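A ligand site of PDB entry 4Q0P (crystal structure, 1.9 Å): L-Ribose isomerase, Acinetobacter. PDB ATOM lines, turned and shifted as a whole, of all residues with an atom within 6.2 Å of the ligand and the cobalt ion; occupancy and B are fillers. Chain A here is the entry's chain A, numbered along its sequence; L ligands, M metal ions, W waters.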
ATOM      1  N   MET A  74      -7.921 -10.445   2.150  1.00  0.00           N
ATOM      2  CA  MET A  74      -9.001 -10.732   1.233  1.00  0.00           C
ATOM      3  C   MET A  74      -9.587 -12.093   1.494  1.00  0.00           C
ATOM      4  O   MET A  74      -9.053 -12.877   2.283  1.00  0.00           O
ATOM      5  CB  MET A  74      -8.490 -10.705  -0.213  1.00  0.00           C
ATOM      6  CG  MET A  74      -7.691 -11.942  -0.576  1.00  0.00           C
ATOM      7  SD  MET A  74      -6.857 -11.757  -2.157  1.00  0.00           S
ATOM      8  CE  MET A  74      -8.258 -11.708  -3.264  1.00  0.00           C
ATOM      9  N   ILE A  76     -11.177 -15.566  -0.507  1.00  0.00           N
ATOM     10  CA  ILE A  76     -11.206 -16.282  -1.767  1.00  0.00           C
ATOM     11  C   ILE A  76     -11.994 -17.574  -1.622  1.00  0.00           C
ATOM     12  O   ILE A  76     -11.721 -18.378  -0.717  1.00  0.00           O
ATOM     13  CB  ILE A  76      -9.791 -16.635  -2.274  1.00  0.00           C
ATOM     14  CG1 ILE A  76      -9.008 -15.348  -2.573  1.00  0.00           C
ATOM     15  CG2 ILE A  76      -9.885 -17.520  -3.510  1.00  0.00           C
ATOM     16  CD1 ILE A  76      -7.611 -15.578  -3.136  1.00  0.00           C
ATOM     17  N   GLU A  78     -12.766 -20.721  -3.808  1.00  0.00           N
ATOM     18  CA  GLU A  78     -12.364 -21.432  -5.006  1.00  0.00           C
ATOM     19  C   GLU A  78     -13.305 -22.566  -5.361  1.00  0.00           C
ATOM     20  O   GLU A  78     -13.443 -23.532  -4.593  1.00  0.00           O
ATOM     21  CB  GLU A  78     -10.942 -21.958  -4.794  1.00  0.00           C
ATOM     22  CG  GLU A  78     -10.371 -22.810  -5.894  1.00  0.00           C
ATOM     23  CD  GLU A  78      -9.001 -23.345  -5.533  1.00  0.00           C
ATOM     24  OE1 GLU A  78      -8.040 -22.537  -5.493  1.00  0.00           O
ATOM     25  OE2 GLU A  78      -8.884 -24.565  -5.271  1.00  0.00           O
ATOM     26  N   CYS A 102      -8.600 -22.729 -12.987  1.00  0.00           N
ATOM     27  CA  CYS A 102      -8.919 -22.340 -11.621  1.00  0.00           C
ATOM     28  C   CYS A 102      -9.967 -21.219 -11.646  1.00  0.00           C
ATOM     29  O   CYS A 102      -9.733 -20.145 -12.220  1.00  0.00           O
ATOM     30  CB  CYS A 102      -7.649 -21.884 -10.889  1.00  0.00           C
ATOM     31  SG  CYS A 102      -7.897 -21.369  -9.173  1.00  0.00           S
ATOM     32  N   LYS A 104     -12.466 -18.898  -9.189  1.00  0.00           N
ATOM     33  CA  LYS A 104     -12.679 -18.499  -7.808  1.00  0.00           C
ATOM     34  C   LYS A 104     -13.343 -17.150  -7.728  1.00  0.00           C
ATOM     35  O   LYS A 104     -13.277 -16.351  -8.671  1.00  0.00           O
ATOM     36  CB  LYS A 104     -11.350 -18.437  -7.053  1.00  0.00           C
ATOM     37  CG  LYS A 104     -10.477 -17.236  -7.437  1.00  0.00           C
ATOM     38  CD  LYS A 104      -9.104 -17.680  -7.965  1.00  0.00           C
ATOM     39  CE  LYS A 104      -9.220 -18.381  -9.309  1.00  0.00           C
ATOM     40  NZ  LYS A 104      -7.877 -18.707  -9.887  1.00  0.00           N
ATOM     41  N   MET A 106     -13.398 -13.709  -5.485  1.00  0.00           N
ATOM     42  CA  MET A 106     -12.552 -13.013  -4.511  1.00  0.00           C
ATOM     43  C   MET A 106     -13.294 -11.803  -3.969  1.00  0.00           C
ATOM     44  O   MET A 106     -13.922 -11.064  -4.728  1.00  0.00           O
ATOM     45  CB  MET A 106     -11.223 -12.599  -5.167  1.00  0.00           C
ATOM     46  CG  MET A 106     -10.428 -13.772  -5.740  1.00  0.00           C
ATOM     47  SD  MET A 106      -8.837 -13.338  -6.512  1.00  0.00           S
ATOM     48  CE  MET A 106      -9.384 -12.117  -7.711  1.00  0.00           C
ATOM     49  N   CYS A 114      -5.100  -6.920  -2.467  1.00  0.00           N
ATOM     50  CA  CYS A 114      -4.591  -8.255  -2.744  1.00  0.00           C
ATOM     51  C   CYS A 114      -3.226  -7.653  -3.099  1.00  0.00           C
ATOM     52  O   CYS A 114      -3.081  -7.011  -4.155  1.00  0.00           O
ATOM     53  CB  CYS A 114      -5.220  -8.884  -3.978  1.00  0.00           C
ATOM     54  SG  CYS A 114      -4.389 -10.432  -4.463  1.00  0.00           S
ATOM     55  N   HIS A 117       2.366  -8.955  -6.288  1.00  0.00           N
ATOM     56  CA  HIS A 117       2.908 -10.296  -6.445  1.00  0.00           C
ATOM     57  C   HIS A 117       2.900 -10.680  -7.924  1.00  0.00           C
ATOM     58  O   HIS A 117       2.357  -9.952  -8.755  1.00  0.00           O
ATOM     59  CB  HIS A 117       2.057 -11.294  -5.667  1.00  0.00           C
ATOM     60  CG  HIS A 117       0.669 -11.474  -6.207  1.00  0.00           C
ATOM     61  ND1 HIS A 117      -0.323 -10.526  -6.053  1.00  0.00           N
ATOM     62  CD2 HIS A 117       0.124 -12.470  -6.941  1.00  0.00           C
ATOM     63  CE1 HIS A 117      -1.425 -10.936  -6.660  1.00  0.00           C
ATOM     64  NE2 HIS A 117      -1.182 -12.109  -7.215  1.00  0.00           N
ATOM     65  N   HIS A 118       3.500 -11.813  -8.232  1.00  0.00           N
ATOM     66  CA  HIS A 118       3.491 -12.306  -9.604  1.00  0.00           C
ATOM     67  C   HIS A 118       3.573 -13.821  -9.592  1.00  0.00           C
ATOM     68  O   HIS A 118       3.924 -14.431  -8.588  1.00  0.00           O
ATOM     69  CB  HIS A 118       4.653 -11.695 -10.424  1.00  0.00           C
ATOM     70  CG  HIS A 118       5.960 -12.401 -10.274  1.00  0.00           C
ATOM     71  ND1 HIS A 118       6.807 -12.177  -9.203  1.00  0.00           N
ATOM     72  CD2 HIS A 118       6.582 -13.310 -11.053  1.00  0.00           C
ATOM     73  CE1 HIS A 118       7.883 -12.926  -9.340  1.00  0.00           C
ATOM     74  NE2 HIS A 118       7.778 -13.621 -10.455  1.00  0.00           N
ATOM     75  N   HIS A 119       3.215 -14.424 -10.713  1.00  0.00           N
ATOM     76  CA  HIS A 119       3.242 -15.874 -10.831  1.00  0.00           C
ATOM     77  C   HIS A 119       4.100 -16.219 -12.036  1.00  0.00           C
ATOM     78  O   HIS A 119       4.066 -15.533 -13.058  1.00  0.00           O
ATOM     79  CB  HIS A 119       1.830 -16.412 -11.068  1.00  0.00           C
ATOM     80  CG  HIS A 119       0.805 -15.813 -10.159  1.00  0.00           C
ATOM     81  ND1 HIS A 119       0.734 -16.115  -8.812  1.00  0.00           N
ATOM     82  CD2 HIS A 119      -0.175 -14.911 -10.395  1.00  0.00           C
ATOM     83  CE1 HIS A 119      -0.252 -15.417  -8.262  1.00  0.00           C
ATOM     84  NE2 HIS A 119      -0.808 -14.676  -9.201  1.00  0.00           N
ATOM     85  N   LYS A 122       0.977 -19.098 -13.535  1.00  0.00           N
ATOM     86  CA  LYS A 122      -0.420 -18.701 -13.637  1.00  0.00           C
ATOM     87  C   LYS A 122      -0.769 -17.400 -14.349  1.00  0.00           C
ATOM     88  O   LYS A 122      -0.258 -16.325 -14.014  1.00  0.00           O
ATOM     89  CB  LYS A 122      -1.047 -18.665 -12.235  1.00  0.00           C
ATOM     90  CG  LYS A 122      -2.536 -18.367 -12.233  1.00  0.00           C
ATOM     91  CD  LYS A 122      -3.150 -18.629 -10.868  1.00  0.00           C
ATOM     92  CE  LYS A 122      -2.591 -17.681  -9.830  1.00  0.00           C
ATOM     93  NZ  LYS A 122      -3.072 -18.028  -8.471  1.00  0.00           N
ATOM     94  N   GLU A 124      -4.032 -15.065 -15.246  1.00  0.00           N
ATOM     95  CA  GLU A 124      -5.377 -14.823 -14.721  1.00  0.00           C
ATOM     96  C   GLU A 124      -6.215 -13.903 -15.610  1.00  0.00           C
ATOM     97  O   GLU A 124      -5.711 -13.240 -16.505  1.00  0.00           O
ATOM     98  CB  GLU A 124      -5.290 -14.163 -13.334  1.00  0.00           C
ATOM     99  CG  GLU A 124      -4.105 -14.599 -12.487  1.00  0.00           C
ATOM    100  CD  GLU A 124      -3.913 -13.753 -11.225  1.00  0.00           C
ATOM    101  OE1 GLU A 124      -4.297 -12.560 -11.198  1.00  0.00           O
ATOM    102  OE2 GLU A 124      -3.355 -14.289 -10.241  1.00  0.00           O
ATOM    103  N   TYR A 126      -9.937 -11.309 -15.087  1.00  0.00           N
ATOM    104  CA  TYR A 126     -10.877 -10.778 -14.118  1.00  0.00           C
ATOM    105  C   TYR A 126     -12.216 -10.377 -14.708  1.00  0.00           C
ATOM    106  O   TYR A 126     -12.290  -9.840 -15.821  1.00  0.00           O
ATOM    107  CB  TYR A 126     -10.310  -9.531 -13.412  1.00  0.00           C
ATOM    108  CG  TYR A 126      -8.886  -9.661 -12.952  1.00  0.00           C
ATOM    109  CD1 TYR A 126      -8.465 -10.745 -12.185  1.00  0.00           C
ATOM    110  CD2 TYR A 126      -7.945  -8.699 -13.308  1.00  0.00           C
ATOM    111  CE1 TYR A 126      -7.137 -10.872 -11.791  1.00  0.00           C
ATOM    112  CE2 TYR A 126      -6.613  -8.817 -12.917  1.00  0.00           C
ATOM    113  CZ  TYR A 126      -6.210  -9.900 -12.164  1.00  0.00           C
ATOM    114  OH  TYR A 126      -4.895 -10.024 -11.809  1.00  0.00           O
ATOM    115  N   MET A 193      -4.416 -10.896 -17.015  1.00  0.00           N
ATOM    116  CA  MET A 193      -3.161 -10.588 -16.342  1.00  0.00           C
ATOM    117  C   MET A 193      -2.232 -11.753 -16.678  1.00  0.00           C
ATOM    118  O   MET A 193      -2.308 -12.828 -16.067  1.00  0.00           O
ATOM    119  CB  MET A 193      -3.352 -10.486 -14.823  1.00  0.00           C
ATOM    120  CG  MET A 193      -2.078 -10.106 -14.047  1.00  0.00           C
ATOM    121  SD  MET A 193      -1.326  -8.507 -14.583  1.00  0.00           S
ATOM    122  CE  MET A 193      -2.638  -7.362 -14.195  1.00  0.00           C
ATOM    123  N   HIS A 199       1.472  -7.704 -10.169  1.00  0.00           N
ATOM    124  CA  HIS A 199       0.138  -7.136 -10.093  1.00  0.00           C
ATOM    125  C   HIS A 199      -0.412  -7.094  -8.684  1.00  0.00           C
ATOM    126  O   HIS A 199       0.035  -7.822  -7.796  1.00  0.00           O
ATOM    127  CB  HIS A 199      -0.834  -7.881 -11.022  1.00  0.00           C
ATOM    128  CG  HIS A 199      -0.956  -9.353 -10.740  1.00  0.00           C
ATOM    129  ND1 HIS A 199       0.057 -10.244 -11.003  1.00  0.00           N
ATOM    130  CD2 HIS A 199      -1.972 -10.074 -10.219  1.00  0.00           C
ATOM    131  CE1 HIS A 199      -0.328 -11.462 -10.659  1.00  0.00           C
ATOM    132  NE2 HIS A 199      -1.553 -11.384 -10.188  1.00  0.00           N
ATOM    133  N   PHE A 201      -4.283  -5.346  -6.556  1.00  0.00           N
ATOM    134  CA  PHE A 201      -5.559  -4.696  -6.767  1.00  0.00           C
ATOM    135  C   PHE A 201      -6.257  -4.413  -5.438  1.00  0.00           C
ATOM    136  O   PHE A 201      -5.972  -5.063  -4.429  1.00  0.00           O
ATOM    137  CB  PHE A 201      -6.453  -5.509  -7.711  1.00  0.00           C
ATOM    138  CG  PHE A 201      -6.796  -6.896  -7.225  1.00  0.00           C
ATOM    139  CD1 PHE A 201      -7.876  -7.113  -6.373  1.00  0.00           C
ATOM    140  CD2 PHE A 201      -6.051  -8.001  -7.651  1.00  0.00           C
ATOM    141  CE1 PHE A 201      -8.226  -8.401  -5.967  1.00  0.00           C
ATOM    142  CE2 PHE A 201      -6.387  -9.292  -7.240  1.00  0.00           C
ATOM    143  CZ  PHE A 201      -7.476  -9.497  -6.397  1.00  0.00           C
ATOM    144  N   GLU A 215     -12.394 -14.725 -10.773  1.00  0.00           N
ATOM    145  CA  GLU A 215     -11.144 -14.923 -11.472  1.00  0.00           C
ATOM    146  C   GLU A 215     -11.128 -16.280 -12.159  1.00  0.00           C
ATOM    147  O   GLU A 215     -11.467 -17.304 -11.554  1.00  0.00           O
ATOM    148  CB  GLU A 215      -9.956 -14.853 -10.516  1.00  0.00           C
ATOM    149  CG  GLU A 215      -8.636 -15.208 -11.202  1.00  0.00           C
ATOM    150  CD  GLU A 215      -7.462 -15.180 -10.255  1.00  0.00           C
ATOM    151  OE1 GLU A 215      -7.160 -14.077  -9.736  1.00  0.00           O
ATOM    152  OE2 GLU A 215      -6.847 -16.238 -10.022  1.00  0.00           O
ATOM    153  N   SER A 217      -8.418 -18.432 -14.150  1.00  0.00           N
ATOM    154  CA  SER A 217      -7.002 -18.493 -14.458  1.00  0.00           C
ATOM    155  C   SER A 217      -6.555 -19.938 -14.665  1.00  0.00           C
ATOM    156  O   SER A 217      -7.363 -20.866 -14.557  1.00  0.00           O
ATOM    157  CB  SER A 217      -6.187 -17.905 -13.306  1.00  0.00           C
ATOM    158  OG  SER A 217      -6.160 -18.800 -12.214  1.00  0.00           O
ATOM    159  N   SER A 220      -3.707 -23.077 -10.038  1.00  0.00           N
ATOM    160  CA  SER A 220      -3.123 -22.295  -8.964  1.00  0.00           C
ATOM    161  C   SER A 220      -2.305 -23.208  -8.045  1.00  0.00           C
ATOM    162  O   SER A 220      -2.859 -23.948  -7.237  1.00  0.00           O
ATOM    163  CB  SER A 220      -4.221 -21.585  -8.173  1.00  0.00           C
ATOM    164  OG  SER A 220      -3.661 -20.766  -7.149  1.00  0.00           O
ATOM    165  N   GLU A 222      -0.525 -23.907  -4.999  1.00  0.00           N
ATOM    166  CA  GLU A 222      -0.425 -23.379  -3.653  1.00  0.00           C
ATOM    167  C   GLU A 222      -0.392 -24.476  -2.588  1.00  0.00           C
ATOM    168  O   GLU A 222      -1.423 -25.048  -2.239  1.00  0.00           O
ATOM    169  CB  GLU A 222      -1.609 -22.439  -3.372  1.00  0.00           C
ATOM    170  CG  GLU A 222      -1.682 -21.248  -4.300  1.00  0.00           C
ATOM    171  CD  GLU A 222      -2.920 -20.388  -4.081  1.00  0.00           C
ATOM    172  OE1 GLU A 222      -4.043 -20.874  -4.375  1.00  0.00           O
ATOM    173  OE2 GLU A 222      -2.775 -19.244  -3.617  1.00  0.00           O
ATOM    174  N   ASN A 243       3.037 -18.392  -6.212  1.00  0.00           N
ATOM    175  CA  ASN A 243       2.578 -17.071  -5.790  1.00  0.00           C
ATOM    176  C   ASN A 243       3.751 -16.339  -5.145  1.00  0.00           C
ATOM    177  O   ASN A 243       4.056 -16.538  -3.971  1.00  0.00           O
ATOM    178  CB  ASN A 243       1.420 -17.177  -4.795  1.00  0.00           C
ATOM    179  CG  ASN A 243       0.207 -17.887  -5.357  1.00  0.00           C
ATOM    180  OD1 ASN A 243      -0.065 -17.811  -6.560  1.00  0.00           O
ATOM    181  ND2 ASN A 243      -0.522 -18.568  -4.497  1.00  0.00           N
ATOM    182  N   PHE A 245       5.094 -13.044  -3.748  1.00  0.00           N
ATOM    183  CA  PHE A 245       4.743 -11.721  -3.265  1.00  0.00           C
ATOM    184  C   PHE A 245       5.988 -10.843  -3.137  1.00  0.00           C
ATOM    185  O   PHE A 245       7.031 -11.309  -2.699  1.00  0.00           O
ATOM    186  CB  PHE A 245       4.002 -11.834  -1.930  1.00  0.00           C
ATOM    187  CG  PHE A 245       2.604 -12.368  -2.074  1.00  0.00           C
ATOM    188  CD1 PHE A 245       1.540 -11.535  -2.404  1.00  0.00           C
ATOM    189  CD2 PHE A 245       2.360 -13.739  -1.929  1.00  0.00           C
ATOM    190  CE1 PHE A 245       0.262 -12.045  -2.608  1.00  0.00           C
ATOM    191  CE2 PHE A 245       1.078 -14.258  -2.130  1.00  0.00           C
ATOM    192  CZ  PHE A 245       0.029 -13.411  -2.470  1.00  0.00           C
ATOM    193  N   ARG A 254       0.521 -15.936   4.459  1.00  0.00           N
ATOM    194  CA  ARG A 254      -0.478 -16.190   3.432  1.00  0.00           C
ATOM    195  C   ARG A 254      -1.007 -17.623   3.509  1.00  0.00           C
ATOM    196  O   ARG A 254      -2.191 -17.876   3.275  1.00  0.00           O
ATOM    197  CB  ARG A 254       0.131 -15.922   2.046  1.00  0.00           C
ATOM    198  CG  ARG A 254      -0.873 -15.788   0.903  1.00  0.00           C
ATOM    199  CD  ARG A 254      -1.522 -17.112   0.539  1.00  0.00           C
ATOM    200  NE  ARG A 254      -2.484 -16.964  -0.548  1.00  0.00           N
ATOM    201  CZ  ARG A 254      -3.230 -17.952  -1.019  1.00  0.00           C
ATOM    202  NH1 ARG A 254      -4.086 -17.711  -2.015  1.00  0.00           N
ATOM    203  NH2 ARG A 254      -3.151 -19.170  -0.493  1.00  0.00           N
HETATM  204  C1  LIG L   1      -4.903 -14.267  -7.637  1.00  0.00           C
HETATM  205  C2  LIG L   1      -5.571 -15.607  -7.340  1.00  0.00           C
HETATM  206  C3  LIG L   1      -5.305 -16.048  -5.896  1.00  0.00           C
HETATM  207  C4  LIG L   1      -3.818 -15.947  -5.514  1.00  0.00           C
HETATM  208  C5  LIG L   1      -3.203 -14.608  -5.942  1.00  0.00           C
HETATM  209  O1  LIG L   1      -5.469 -13.262  -6.810  1.00  0.00           O
HETATM  210  O2  LIG L   1      -5.111 -16.590  -8.253  1.00  0.00           O
HETATM  211  O3  LIG L   1      -5.740 -17.386  -5.733  1.00  0.00           O
HETATM  212  O4  LIG L   1      -3.083 -17.022  -6.096  1.00  0.00           O
HETATM  213  O5  LIG L   1      -3.487 -14.343  -7.327  1.00  0.00           O
HETATM  214 CO    CO M   1      -2.259 -13.042  -8.982  1.00  0.00          CO
HETATM  215  O   HOH W   1      -3.958 -11.704  -8.619  1.00  0.00           O
HETATM  216  O   HOH W   2      -7.216 -19.909  -6.082  1.00  0.00           O
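Water W1 bridges the side-chain carboxylate (OE1) of Glu 124 (2.7 Å) and an oxygen (O1) of the ligand (2.8 Å).
Water W2 lies within hydrogen-bond range of the side-chain carboxylate of Glu 78, an oxygen (O3) of the ligand and the side-chain sulfur of Cys 102.
Residues that only touch the ligand: Ile 76 (3.6 Å), Cys 114 (3.8 Å), Lys 104 (3.8 Å), Arg 254 (3.9 Å) and Ser 220 (3.9 Å).
Hydrophobic or aromatic side chains within 4 Å of the ligand: Ile 76, Met 106 and His 119.
Within 4 Å of the ligand: Ile 76, Lys 104, Met 106, Cys 114, His 117, His 119, Lys 122, Glu 124, Glu 215, Ser 220, Glu 222, Asn 243 and Arg 254.
The cobalt ion is bound by the side-chain carboxylate of Glu 124 (2.1 Å), a ring nitrogen (NE2) of His 199 (2.2 Å), water W1 (2.2 Å), a ring nitrogen (NE2) of His 119 (2.2 Å), a ring nitrogen (NE2) of His 117 (2.3 Å) and an oxygen (O5) of the ligand (2.4 Å).
The cobalt ion has six donor atoms within binding distance.
The side-chain carboxylate of Glu 124 lies within hydrogen-bond range of the side-chain hydroxyl of Tyr 126, at 2.7 Å.
The backbone NH (N) of Met 193 sits at hydrogen-bond distance from the backbone carbonyl oxygen (O) of Glu 124 (2.7 Å).
OE2 of Glu 215 lies within salt-bridge range of NZ of Lys 104, at 2.7 Å.
The side-chain carboxylate of Glu 215 sits at hydrogen-bond distance from the side-chain hydroxyl of Ser 217 (3.4 Å).
The side-chain amide nitrogen (ND2) of Asn 243 lies within hydrogen-bond range of the side-chain carboxylate (OE2) of Glu 222 (2.5 Å).
The side-chain carboxylate of Glu 222 lies within salt-bridge range of the guanidinium group of Arg 254 (2.6 Å).
N of Cys 114 is in hydrogen-bond range of O of Phe 201 (2.8 Å).
The side-chain amino group (NZ) of Lys 104 sits at hydrogen-bond distance from the side-chain sulfur (SG) of Cys 102 (2.8 Å).
The side-chain carboxylate (OE2) of Glu 215 lies within hydrogen-bond range of an oxygen (O2) of the ligand, at 2.5 Å.
An oxygen (O2) of the ligand sits at hydrogen-bond distance from the side-chain amino group (NZ) of Lys 122 (2.5 Å).
An oxygen (O4) of the ligand is in hydrogen-bond range of the side-chain amide oxygen (OD1) of Asn 243, 3.2 Å away.
O4 of the ligand sits at hydrogen-bond distance from OE2 of Glu 222 (3.3 Å).
The side-chain sulfur (SD) of Met 106 is in hydrogen-bond range of an oxygen (O1) of the ligand, 3.4 Å away.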
